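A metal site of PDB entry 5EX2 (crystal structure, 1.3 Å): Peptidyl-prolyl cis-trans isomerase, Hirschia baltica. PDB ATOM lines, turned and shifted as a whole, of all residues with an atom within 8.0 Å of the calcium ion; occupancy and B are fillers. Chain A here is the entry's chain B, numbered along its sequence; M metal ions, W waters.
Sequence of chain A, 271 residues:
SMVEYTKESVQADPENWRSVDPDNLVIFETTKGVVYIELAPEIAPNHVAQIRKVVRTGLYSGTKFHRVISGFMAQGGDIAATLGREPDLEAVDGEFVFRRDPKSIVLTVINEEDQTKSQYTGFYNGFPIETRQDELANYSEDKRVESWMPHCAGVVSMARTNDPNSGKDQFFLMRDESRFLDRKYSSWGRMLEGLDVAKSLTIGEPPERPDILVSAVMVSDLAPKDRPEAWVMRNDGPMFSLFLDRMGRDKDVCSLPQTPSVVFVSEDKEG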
ATOM      1  N   VAL A 109     -26.203 -30.549  25.635  1.00  0.00           N
ATOM      2  CA  VAL A 109     -25.567 -29.279  25.306  1.00  0.00           C
ATOM      3  C   VAL A 109     -24.390 -29.039  26.222  1.00  0.00           C
ATOM      4  O   VAL A 109     -24.280 -29.617  27.295  1.00  0.00           O
ATOM      5  CB  VAL A 109     -26.568 -28.111  25.399  1.00  0.00           C
ATOM      6  CG1 VAL A 109     -27.730 -28.390  24.485  1.00  0.00           C
ATOM      7  CG2 VAL A 109     -27.047 -27.928  26.840  1.00  0.00           C
ATOM      8  N   ASP A 114     -29.126 -19.566  26.704  1.00  0.00           N
ATOM      9  CA  ASP A 114     -30.038 -19.513  25.564  1.00  0.00           C
ATOM     10  C   ASP A 114     -29.245 -19.521  24.252  1.00  0.00           C
ATOM     11  O   ASP A 114     -28.291 -18.762  24.095  1.00  0.00           O
ATOM     12  CB  ASP A 114     -30.936 -18.281  25.610  1.00  0.00           C
ATOM     13  CG  ASP A 114     -31.839 -18.233  26.822  1.00  0.00           C
ATOM     14  OD1 ASP A 114     -32.022 -19.279  27.484  1.00  0.00           O
ATOM     15  OD2 ASP A 114     -32.381 -17.150  27.106  1.00  0.00           O
ATOM     16  N   GLN A 115     -29.641 -20.380  23.334  1.00  0.00           N
ATOM     17  CA  GLN A 115     -29.010 -20.461  22.019  1.00  0.00           C
ATOM     18  C   GLN A 115     -29.396 -19.281  21.139  1.00  0.00           C
ATOM     19  O   GLN A 115     -30.534 -18.830  21.180  1.00  0.00           O
ATOM     20  CB  GLN A 115     -29.411 -21.772  21.358  1.00  0.00           C
ATOM     21  CG  GLN A 115     -28.838 -23.008  22.052  1.00  0.00           C
ATOM     22  CD  GLN A 115     -29.481 -24.284  21.592  1.00  0.00           C
ATOM     23  OE1 GLN A 115     -30.491 -24.266  20.904  1.00  0.00           O
ATOM     24  NE2 GLN A 115     -28.881 -25.407  21.961  1.00  0.00           N
ATOM     25  N   THR A 116     -28.465 -18.800  20.320  1.00  0.00           N
ATOM     26  CA  THR A 116     -28.732 -17.688  19.417  1.00  0.00           C
ATOM     27  C   THR A 116     -28.154 -17.919  18.021  1.00  0.00           C
ATOM     28  O   THR A 116     -28.128 -17.007  17.216  1.00  0.00           O
ATOM     29  CB  THR A 116     -28.130 -16.370  19.945  1.00  0.00           C
ATOM     30  OG1 THR A 116     -26.704 -16.497  20.059  1.00  0.00           O
ATOM     31  CG2 THR A 116     -28.735 -15.987  21.286  1.00  0.00           C
ATOM     32  N   LYS A 117     -27.642 -19.097  17.744  1.00  0.00           N
ATOM     33  CA  LYS A 117     -26.994 -19.338  16.465  1.00  0.00           C
ATOM     34  C   LYS A 117     -27.820 -20.295  15.607  1.00  0.00           C
ATOM     35  O   LYS A 117     -28.750 -20.951  16.080  1.00  0.00           O
ATOM     36  CB  LYS A 117     -25.594 -19.903  16.707  1.00  0.00           C
ATOM     37  CG  LYS A 117     -24.675 -18.926  17.439  1.00  0.00           C
ATOM     38  CD  LYS A 117     -23.261 -19.449  17.575  1.00  0.00           C
ATOM     39  CE  LYS A 117     -22.407 -18.535  18.463  1.00  0.00           C
ATOM     40  NZ  LYS A 117     -20.985 -18.969  18.547  1.00  0.00           N
ATOM     41  N   SER A 118     -27.443 -20.401  14.338  1.00  0.00           N
ATOM     42  CA  SER A 118     -28.123 -21.323  13.427  1.00  0.00           C
ATOM     43  C   SER A 118     -27.790 -22.780  13.703  1.00  0.00           C
ATOM     44  O   SER A 118     -28.519 -23.682  13.298  1.00  0.00           O
ATOM     45  CB  SER A 118     -27.760 -20.984  11.994  1.00  0.00           C
ATOM     46  OG  SER A 118     -28.298 -19.728  11.634  1.00  0.00           O
ATOM     47  N   GLN A 119     -26.672 -23.009  14.364  1.00  0.00           N
ATOM     48  CA  GLN A 119     -26.241 -24.356  14.689  1.00  0.00           C
ATOM     49  C   GLN A 119     -25.719 -24.387  16.103  1.00  0.00           C
ATOM     50  O   GLN A 119     -25.383 -23.369  16.679  1.00  0.00           O
ATOM     51  CB  GLN A 119     -25.153 -24.820  13.701  1.00  0.00           C
ATOM     52  CG  GLN A 119     -25.697 -24.969  12.299  1.00  0.00           C
ATOM     53  CD  GLN A 119     -24.665 -25.146  11.181  1.00  0.00           C
ATOM     54  OE1 GLN A 119     -25.056 -25.090  10.028  1.00  0.00           O
ATOM     55  NE2 GLN A 119     -23.400 -25.407  11.521  1.00  0.00           N
ATOM     56  N   TYR A 120     -25.653 -25.584  16.683  1.00  0.00           N
ATOM     57  CA  TYR A 120     -24.949 -25.729  17.943  1.00  0.00           C
ATOM     58  C   TYR A 120     -24.375 -27.127  17.973  1.00  0.00           C
ATOM     59  O   TYR A 120     -24.696 -27.963  17.130  1.00  0.00           O
ATOM     60  CB  TYR A 120     -25.859 -25.488  19.148  1.00  0.00           C
ATOM     61  CG  TYR A 120     -26.922 -26.530  19.367  1.00  0.00           C
ATOM     62  CD1 TYR A 120     -28.149 -26.437  18.723  1.00  0.00           C
ATOM     63  CD2 TYR A 120     -26.704 -27.604  20.231  1.00  0.00           C
ATOM     64  CE1 TYR A 120     -29.127 -27.404  18.927  1.00  0.00           C
ATOM     65  CE2 TYR A 120     -27.662 -28.553  20.427  1.00  0.00           C
ATOM     66  CZ  TYR A 120     -28.869 -28.470  19.788  1.00  0.00           C
ATOM     67  OH  TYR A 120     -29.815 -29.448  20.000  1.00  0.00           O
ATOM     68  N   THR A 131     -25.586 -29.658  14.835  1.00  0.00           N
ATOM     69  CA  THR A 131     -26.946 -29.755  14.383  1.00  0.00           C
ATOM     70  C   THR A 131     -27.519 -28.397  14.015  1.00  0.00           C
ATOM     71  O   THR A 131     -27.132 -27.374  14.556  1.00  0.00           O
ATOM     72  CB  THR A 131     -27.832 -30.405  15.454  1.00  0.00           C
ATOM     73  OG1 THR A 131     -29.130 -30.657  14.932  1.00  0.00           O
ATOM     74  CG2 THR A 131     -27.918 -29.540  16.705  1.00  0.00           C
ATOM     75  N   ARG A 132     -28.399 -28.428  13.027  1.00  0.00           N
ATOM     76  CA  ARG A 132     -29.316 -27.336  12.814  1.00  0.00           C
ATOM     77  C   ARG A 132     -30.292 -27.311  13.987  1.00  0.00           C
ATOM     78  O   ARG A 132     -30.410 -28.263  14.738  1.00  0.00           O
ATOM     79  CB  ARG A 132     -30.039 -27.498  11.483  1.00  0.00           C
ATOM     80  CG  ARG A 132     -29.082 -27.630  10.295  1.00  0.00           C
ATOM     81  CD  ARG A 132     -28.278 -26.376  10.040  1.00  0.00           C
ATOM     82  NE  ARG A 132     -29.113 -25.319   9.455  1.00  0.00           N
ATOM     83  CZ  ARG A 132     -28.672 -24.114   9.135  1.00  0.00           C
ATOM     84  NH1 ARG A 132     -27.406 -23.784   9.329  1.00  0.00           N
ATOM     85  NH2 ARG A 132     -29.511 -23.234   8.594  1.00  0.00           N
ATOM     86  N   GLN A 133     -30.988 -26.199  14.162  1.00  0.00           N
ATOM     87  CA  GLN A 133     -31.779 -26.014  15.371  1.00  0.00           C
ATOM     88  C   GLN A 133     -32.988 -26.939  15.472  1.00  0.00           C
ATOM     89  O   GLN A 133     -33.717 -27.145  14.501  1.00  0.00           O
ATOM     90  CB  GLN A 133     -32.235 -24.569  15.453  1.00  0.00           C
ATOM     91  CG  GLN A 133     -31.139 -23.626  15.865  1.00  0.00           C
ATOM     92  CD  GLN A 133     -30.673 -23.865  17.289  1.00  0.00           C
ATOM     93  OE1 GLN A 133     -31.296 -24.620  18.046  1.00  0.00           O
ATOM     94  NE2 GLN A 133     -29.613 -23.205  17.666  1.00  0.00           N
ATOM     95  N   ASP A 134     -33.217 -27.459  16.669  1.00  0.00           N
ATOM     96  CA  ASP A 134     -34.283 -28.423  16.884  1.00  0.00           C
ATOM     97  C   ASP A 134     -35.638 -27.857  16.581  1.00  0.00           C
ATOM     98  O   ASP A 134     -36.559 -28.595  16.208  1.00  0.00           O
ATOM     99  CB  ASP A 134     -34.242 -28.914  18.332  1.00  0.00           C
ATOM    100  CG  ASP A 134     -32.874 -29.460  18.717  1.00  0.00           C
ATOM    101  OD1 ASP A 134     -31.992 -28.648  19.058  1.00  0.00           O
ATOM    102  OD2 ASP A 134     -32.687 -30.703  18.684  1.00  0.00           O
ATOM    103  N   GLU A 135     -35.781 -26.552  16.727  1.00  0.00           N
ATOM    104  CA  GLU A 135     -37.053 -25.902  16.480  1.00  0.00           C
ATOM    105  C   GLU A 135     -37.518 -26.126  15.036  1.00  0.00           C
ATOM    106  O   GLU A 135     -38.717 -26.048  14.754  1.00  0.00           O
ATOM    107  CB  GLU A 135     -36.971 -24.408  16.817  1.00  0.00           C
ATOM    108  CG  GLU A 135     -36.784 -24.082  18.314  1.00  0.00           C
ATOM    109  CD  GLU A 135     -35.375 -24.251  18.842  1.00  0.00           C
ATOM    110  OE1 GLU A 135     -34.444 -24.394  18.042  1.00  0.00           O
ATOM    111  OE2 GLU A 135     -35.179 -24.254  20.074  1.00  0.00           O
ATOM    112  N   LEU A 136     -36.609 -26.403  14.116  1.00  0.00           N
ATOM    113  CA  LEU A 136     -37.005 -26.635  12.731  1.00  0.00           C
ATOM    114  C   LEU A 136     -37.842 -27.906  12.585  1.00  0.00           C
ATOM    115  O   LEU A 136     -38.627 -28.041  11.630  1.00  0.00           O
ATOM    116  CB  LEU A 136     -35.773 -26.724  11.811  1.00  0.00           C
ATOM    117  CG  LEU A 136     -34.832 -25.530  11.785  1.00  0.00           C
ATOM    118  CD1 LEU A 136     -33.740 -25.791  10.763  1.00  0.00           C
ATOM    119  CD2 LEU A 136     -35.568 -24.251  11.502  1.00  0.00           C
HETATM  120 CA    CA M   1     -32.691 -24.282  19.929  1.00  0.00          CA
HETATM  121  O   HOH W   1     -32.639 -21.978  19.491  1.00  0.00           O
HETATM  122  O   HOH W   2     -32.705 -26.544  20.493  1.00  0.00           O
HETATM  123  O   HOH W   3     -33.238 -23.666  22.159  1.00  0.00           O
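The side-chain amide nitrogen (NE2) of Gln 133 is in hydrogen-bond range of the backbone carbonyl oxygen (O) of Lys 117 (2.9 Å).
Three residues have an atom within 4 Å of the calcium ion: Gln 115, Gln 133 and Glu 135.
The nearest printed residue that does not touch the calcium ion is Asp 134 (4.5 Å).
The calcium ion is bound by water W2 (2.3 Å), water W1 (2.3 Å), OE1 of Gln 133 (2.4 Å), water W3 (2.4 Å), OE1 of Gln 115 (2.4 Å), OE2 of Glu 135 (2.5 Å) and OE1 of Glu 135 (2.6 Å).
The calcium ion has seven donor atoms within binding distance.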
